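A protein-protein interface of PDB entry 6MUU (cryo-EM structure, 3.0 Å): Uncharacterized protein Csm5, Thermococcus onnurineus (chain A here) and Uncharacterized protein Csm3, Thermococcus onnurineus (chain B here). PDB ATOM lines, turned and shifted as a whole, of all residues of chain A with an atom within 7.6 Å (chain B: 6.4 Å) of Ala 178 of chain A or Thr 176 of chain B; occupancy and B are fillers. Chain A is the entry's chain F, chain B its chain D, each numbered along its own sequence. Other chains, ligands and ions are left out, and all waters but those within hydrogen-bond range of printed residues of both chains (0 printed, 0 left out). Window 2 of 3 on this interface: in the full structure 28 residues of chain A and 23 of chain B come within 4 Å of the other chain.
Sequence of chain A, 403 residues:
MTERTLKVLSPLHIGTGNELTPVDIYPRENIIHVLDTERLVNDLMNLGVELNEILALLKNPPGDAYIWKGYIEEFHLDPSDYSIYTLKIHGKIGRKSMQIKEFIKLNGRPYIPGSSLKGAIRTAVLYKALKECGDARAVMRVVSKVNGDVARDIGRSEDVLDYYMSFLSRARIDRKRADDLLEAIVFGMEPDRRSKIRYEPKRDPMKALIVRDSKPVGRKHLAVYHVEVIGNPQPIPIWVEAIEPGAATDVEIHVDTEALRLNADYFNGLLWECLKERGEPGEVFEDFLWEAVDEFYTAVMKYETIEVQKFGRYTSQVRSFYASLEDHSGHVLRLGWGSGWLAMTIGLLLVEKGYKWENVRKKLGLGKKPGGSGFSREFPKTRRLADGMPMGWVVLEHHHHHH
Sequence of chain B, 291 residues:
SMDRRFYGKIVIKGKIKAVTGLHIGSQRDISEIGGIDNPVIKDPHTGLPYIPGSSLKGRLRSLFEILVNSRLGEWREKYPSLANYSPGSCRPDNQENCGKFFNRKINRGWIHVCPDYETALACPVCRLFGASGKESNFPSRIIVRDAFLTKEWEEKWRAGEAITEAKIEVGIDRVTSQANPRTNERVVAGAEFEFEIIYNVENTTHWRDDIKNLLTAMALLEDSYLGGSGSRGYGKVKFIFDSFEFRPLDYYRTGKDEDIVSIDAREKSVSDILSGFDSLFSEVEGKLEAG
The backbone carbonyl oxygen of Val 175 of chain B is in hydrogen-bond range of the indole nitrogen of Trp 341 of chain A, at 3.3 Å.
O of Arg 174 of chain B sits close to OG1 of Thr 345 of chain A, at 3.4 Å.
The side-chain carboxylate (OD1) of Asp 173 of chain B sits at hydrogen-bond distance from the backbone NH (N) of Asp 179 of chain A, 2.6 Å away.
O of Lys 176 of chain A sits close to OD2 of Asp 173 of chain B (3.0 Å).
The backbone NH (N) of Ala 178 of chain A lies within hydrogen-bond range of the side-chain carboxylate (OD2) of Asp 173 of chain B (2.8 Å).
Arg 175 of chain A touches Gln 178 of chain B (N to CB, 3.4 Å).
OG1 of Thr 176 of chain B touches CB of Lys 176 of chain A (3.4 Å).
Gln 178 of chain B touches Lys 176 of chain A (CB to N, 3.9 Å).
Arg 177 of chain A touches Asp 173 of chain B.
Ala 178 of chain A touches Val 175 of chain B (CB to CB, 3.7 Å).
CB of Ala 178 of chain A touches CG2 of Thr 176 of chain B, at 3.8 Å.
Asp 179 of chain A touches Arg 174 of chain B (CB to N, 3.5 Å).
Trp 341 of chain A touches Ser 177 of chain B.
CG2 of Thr 345 of chain A touches O of Val 175 of chain B (3.98 Å).
Leu 168 of chain A touches none of the printed residues of chain B.
Of the printed residues of chain B, Arg 175 of chain A touches Gln 178 (3.4 Å).
Printed residues of chain B within 4 Å of Lys 176 of chain A: Asp 173, Thr 176 and Gln 178.
Ala 178 of chain A touches just these residues of chain B: Asp 173 (2.8 Å), Val 175 (3.7 Å) and Thr 176 (3.8 Å).
Leu 181 of chain A touches none of the printed residues of chain B.
Of the printed residues of chain A, Ser 177 of chain B touches Trp 341.
OG1 of Thr 345 of chain A is in hydrogen-bond range of O of Trp 341 of chain A.
The backbone NH (N) of Asp 173 of chain B sits at hydrogen-bond distance from the backbone carbonyl oxygen (O) of Gln 178 of chain B (3.1 Å).
The side-chain hydroxyl of Thr 176 of chain B is in hydrogen-bond range of the side-chain carboxylate of Asp 173 of chain B (2.6 Å).
Hydrophobic or aromatic side chains of chain B within 4 Å of the printed part of chain A: Val 175.
Of the 15 printed residues of chain A, 7 touch a printed residue of chain B.
Among the printed residues, no Asp or Glu carboxylate lies within 4 Å of a Lys or Arg side-chain nitrogen of the other chain.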
ATOM      1  N   TYR A 164     -10.225 -25.336  29.231  1.00  0.00           N
ATOM      2  CA  TYR A 164      -9.525 -25.200  27.962  1.00  0.00           C
ATOM      3  C   TYR A 164     -10.470 -25.010  26.785  1.00  0.00           C
ATOM      4  O   TYR A 164     -10.048 -24.485  25.749  1.00  0.00           O
ATOM      5  CB  TYR A 164      -8.636 -26.422  27.719  1.00  0.00           C
ATOM      6  N   LEU A 168      -9.751 -22.140  24.334  1.00  0.00           N
ATOM      7  CA  LEU A 168      -9.576 -22.284  22.894  1.00  0.00           C
ATOM      8  C   LEU A 168     -10.559 -21.413  22.123  1.00  0.00           C
ATOM      9  O   LEU A 168     -10.276 -21.018  20.986  1.00  0.00           O
ATOM     10  CB  LEU A 168      -9.727 -23.748  22.487  1.00  0.00           C
ATOM     11  N   ARG A 175       1.368 -26.133  12.544  1.00  0.00           N
ATOM     12  CA  ARG A 175       1.095 -24.723  12.299  1.00  0.00           C
ATOM     13  C   ARG A 175       0.121 -24.169  13.333  1.00  0.00           C
ATOM     14  O   ARG A 175      -0.581 -23.189  13.080  1.00  0.00           O
ATOM     15  CB  ARG A 175       0.551 -24.525  10.897  1.00  0.00           C
ATOM     16  N   LYS A 176       0.078 -24.804  14.500  1.00  0.00           N
ATOM     17  CA  LYS A 176      -0.768 -24.338  15.587  1.00  0.00           C
ATOM     18  C   LYS A 176      -0.075 -24.625  16.910  1.00  0.00           C
ATOM     19  O   LYS A 176       0.701 -25.577  17.029  1.00  0.00           O
ATOM     20  CB  LYS A 176      -2.155 -24.991  15.542  1.00  0.00           C
ATOM     21  N   ARG A 177      -0.363 -23.789  17.903  1.00  0.00           N
ATOM     22  CA  ARG A 177       0.251 -23.869  19.222  1.00  0.00           C
ATOM     23  C   ARG A 177      -0.785 -24.157  20.304  1.00  0.00           C
ATOM     24  O   ARG A 177      -0.802 -23.514  21.355  1.00  0.00           O
ATOM     25  CB  ARG A 177       1.015 -22.586  19.540  1.00  0.00           C
ATOM     26  N   ALA A 178      -1.676 -25.116  20.051  1.00  0.00           N
ATOM     27  CA  ALA A 178      -2.724 -25.420  21.018  1.00  0.00           C
ATOM     28  C   ALA A 178      -2.197 -26.199  22.217  1.00  0.00           C
ATOM     29  O   ALA A 178      -2.771 -26.107  23.307  1.00  0.00           O
ATOM     30  CB  ALA A 178      -3.857 -26.188  20.340  1.00  0.00           C
ATOM     31  N   ASP A 179      -1.124 -26.969  22.047  1.00  0.00           N
ATOM     32  CA  ASP A 179      -0.467 -27.619  23.173  1.00  0.00           C
ATOM     33  C   ASP A 179       0.588 -26.740  23.826  1.00  0.00           C
ATOM     34  O   ASP A 179       1.268 -27.199  24.747  1.00  0.00           O
ATOM     35  CB  ASP A 179       0.176 -28.940  22.739  1.00  0.00           C
ATOM     36  N   ASP A 180       0.751 -25.497  23.369  1.00  0.00           N
ATOM     37  CA  ASP A 180       1.720 -24.608  23.998  1.00  0.00           C
ATOM     38  C   ASP A 180       1.241 -24.137  25.361  1.00  0.00           C
ATOM     39  O   ASP A 180       2.061 -23.779  26.212  1.00  0.00           O
ATOM     40  CB  ASP A 180       2.008 -23.407  23.098  1.00  0.00           C
ATOM     41  N   LEU A 181      -0.072 -24.123  25.586  1.00  0.00           N
ATOM     42  CA  LEU A 181      -0.618 -23.736  26.879  1.00  0.00           C
ATOM     43  C   LEU A 181      -0.932 -24.928  27.769  1.00  0.00           C
ATOM     44  O   LEU A 181      -0.768 -24.837  28.990  1.00  0.00           O
ATOM     45  CB  LEU A 181      -1.881 -22.896  26.686  1.00  0.00           C
ATOM     46  N   LEU A 182      -1.376 -26.044  27.190  1.00  0.00           N
ATOM     47  CA  LEU A 182      -1.762 -27.195  27.996  1.00  0.00           C
ATOM     48  C   LEU A 182      -0.547 -27.934  28.544  1.00  0.00           C
ATOM     49  O   LEU A 182      -0.553 -28.355  29.706  1.00  0.00           O
ATOM     50  CB  LEU A 182      -2.641 -28.143  27.178  1.00  0.00           C
ATOM     51  N   GLU A 183       0.498 -28.101  27.732  1.00  0.00           N
ATOM     52  CA  GLU A 183       1.717 -28.742  28.209  1.00  0.00           C
ATOM     53  C   GLU A 183       2.536 -27.837  29.119  1.00  0.00           C
ATOM     54  O   GLU A 183       3.302 -28.346  29.942  1.00  0.00           O
ATOM     55  CB  GLU A 183       2.578 -29.198  27.031  1.00  0.00           C
ATOM     56  N   TRP A 341      -5.691 -39.765  14.876  1.00  0.00           N
ATOM     57  CA  TRP A 341      -5.641 -38.503  15.659  1.00  0.00           C
ATOM     58  C   TRP A 341      -5.947 -38.801  17.132  1.00  0.00           C
ATOM     59  O   TRP A 341      -5.241 -38.239  17.991  1.00  0.00           O
ATOM     60  CB  TRP A 341      -6.629 -37.481  15.085  1.00  0.00           C
ATOM     61  CG  TRP A 341      -6.786 -36.263  15.939  1.00  0.00           C
ATOM     62  CD1 TRP A 341      -6.111 -35.083  15.820  1.00  0.00           C
ATOM     63  CD2 TRP A 341      -7.672 -36.105  17.062  1.00  0.00           C
ATOM     64  NE1 TRP A 341      -6.520 -34.202  16.784  1.00  0.00           N
ATOM     65  CE2 TRP A 341      -7.477 -34.800  17.559  1.00  0.00           C
ATOM     66  CE3 TRP A 341      -8.613 -36.930  17.688  1.00  0.00           C
ATOM     67  CZ2 TRP A 341      -8.188 -34.308  18.654  1.00  0.00           C
ATOM     68  CZ3 TRP A 341      -9.310 -36.444  18.770  1.00  0.00           C
ATOM     69  CH2 TRP A 341      -9.100 -35.150  19.245  1.00  0.00           C
ATOM     70  N   THR A 345      -3.705 -37.890  20.606  1.00  0.00           N
ATOM     71  CA  THR A 345      -4.422 -36.747  21.158  1.00  0.00           C
ATOM     72  C   THR A 345      -5.073 -37.170  22.473  1.00  0.00           C
ATOM     73  O   THR A 345      -5.327 -38.353  22.711  1.00  0.00           O
ATOM     74  CB  THR A 345      -5.455 -36.245  20.117  1.00  0.00           C
ATOM     75  OG1 THR A 345      -4.796 -36.042  18.861  1.00  0.00           O
ATOM     76  CG2 THR A 345      -6.141 -34.924  20.487  1.00  0.00           C
ATOM     77  N   VAL A 360     -15.560 -27.815  20.147  1.00  0.00           N
ATOM     78  CA  VAL A 360     -14.203 -27.337  19.915  1.00  0.00           C
ATOM     79  C   VAL A 360     -13.639 -27.858  18.598  1.00  0.00           C
ATOM     80  O   VAL A 360     -12.994 -27.108  17.858  1.00  0.00           O
ATOM     81  CB  VAL A 360     -13.298 -27.738  21.081  1.00  0.00           C
ATOM     82  N   LEU A 364     -11.977 -26.045  15.290  1.00  0.00           N
ATOM     83  CA  LEU A 364     -10.559 -26.332  15.092  1.00  0.00           C
ATOM     84  C   LEU A 364     -10.348 -27.346  13.976  1.00  0.00           C
ATOM     85  O   LEU A 364      -9.274 -27.405  13.375  1.00  0.00           O
ATOM     86  CB  LEU A 364      -9.935 -26.833  16.383  1.00  0.00           C
ATOM     87  N   ASP B 173       1.651 -30.581  17.589  1.00  0.00           N
ATOM     88  CA  ASP B 173       0.644 -29.984  18.459  1.00  0.00           C
ATOM     89  C   ASP B 173      -0.346 -31.056  18.896  1.00  0.00           C
ATOM     90  O   ASP B 173      -0.890 -31.783  18.066  1.00  0.00           O
ATOM     91  CB  ASP B 173      -0.074 -28.861  17.703  1.00  0.00           C
ATOM     92  CG  ASP B 173      -0.973 -28.014  18.588  1.00  0.00           C
ATOM     93  OD1 ASP B 173      -1.046 -28.237  19.810  1.00  0.00           O
ATOM     94  OD2 ASP B 173      -1.633 -27.111  18.041  1.00  0.00           O
ATOM     95  N   ARG B 174      -0.578 -31.158  20.204  1.00  0.00           N
ATOM     96  CA  ARG B 174      -1.342 -32.290  20.717  1.00  0.00           C
ATOM     97  C   ARG B 174      -2.825 -32.165  20.397  1.00  0.00           C
ATOM     98  O   ARG B 174      -3.468 -33.155  20.042  1.00  0.00           O
ATOM     99  CB  ARG B 174      -1.127 -32.430  22.221  1.00  0.00           C
ATOM    100  CG  ARG B 174       0.284 -32.832  22.596  1.00  0.00           C
ATOM    101  CD  ARG B 174       0.566 -34.269  22.197  1.00  0.00           C
ATOM    102  NE  ARG B 174       1.884 -34.709  22.635  1.00  0.00           N
ATOM    103  CZ  ARG B 174       2.981 -34.621  21.892  1.00  0.00           C
ATOM    104  NH1 ARG B 174       4.141 -35.047  22.365  1.00  0.00           N
ATOM    105  NH2 ARG B 174       2.918 -34.101  20.676  1.00  0.00           N
ATOM    106  N   VAL B 175      -3.379 -30.957  20.480  1.00  0.00           N
ATOM    107  CA  VAL B 175      -4.827 -30.804  20.385  1.00  0.00           C
ATOM    108  C   VAL B 175      -5.282 -30.756  18.929  1.00  0.00           C
ATOM    109  O   VAL B 175      -6.219 -31.460  18.535  1.00  0.00           O
ATOM    110  CB  VAL B 175      -5.277 -29.556  21.168  1.00  0.00           C
ATOM    111  CG1 VAL B 175      -6.780 -29.348  21.031  1.00  0.00           C
ATOM    112  CG2 VAL B 175      -4.887 -29.688  22.629  1.00  0.00           C
ATOM    113  N   THR B 176      -4.625 -29.944  18.102  1.00  0.00           N
ATOM    114  CA  THR B 176      -5.057 -29.750  16.723  1.00  0.00           C
ATOM    115  C   THR B 176      -4.352 -30.661  15.726  1.00  0.00           C
ATOM    116  O   THR B 176      -4.731 -30.660  14.549  1.00  0.00           O
ATOM    117  CB  THR B 176      -4.848 -28.293  16.299  1.00  0.00           C
ATOM    118  OG1 THR B 176      -3.454 -27.970  16.366  1.00  0.00           O
ATOM    119  CG2 THR B 176      -5.625 -27.359  17.207  1.00  0.00           C
ATOM    120  N   SER B 177      -3.328 -31.404  16.166  1.00  0.00           N
ATOM    121  CA  SER B 177      -2.562 -32.369  15.360  1.00  0.00           C
ATOM    122  C   SER B 177      -1.880 -31.725  14.153  1.00  0.00           C
ATOM    123  O   SER B 177      -1.592 -32.395  13.160  1.00  0.00           O
ATOM    124  CB  SER B 177      -3.423 -33.559  14.925  1.00  0.00           C
ATOM    125  OG  SER B 177      -2.652 -34.497  14.195  1.00  0.00           O
ATOM    126  N   GLN B 178      -1.602 -30.428  14.228  1.00  0.00           N
ATOM    127  CA  GLN B 178      -0.841 -29.744  13.197  1.00  0.00           C
ATOM    128  C   GLN B 178       0.643 -29.927  13.471  1.00  0.00           C
ATOM    129  O   GLN B 178       1.076 -29.941  14.626  1.00  0.00           O
ATOM    130  CB  GLN B 178      -1.199 -28.258  13.153  1.00  0.00           C
ATOM    131  CG  GLN B 178      -2.648 -27.986  12.788  1.00  0.00           C
ATOM    132  CD  GLN B 178      -2.979 -28.397  11.369  1.00  0.00           C
ATOM    133  OE1 GLN B 178      -2.182 -28.201  10.452  1.00  0.00           O
ATOM    134  NE2 GLN B 178      -4.157 -28.978  11.182  1.00  0.00           N
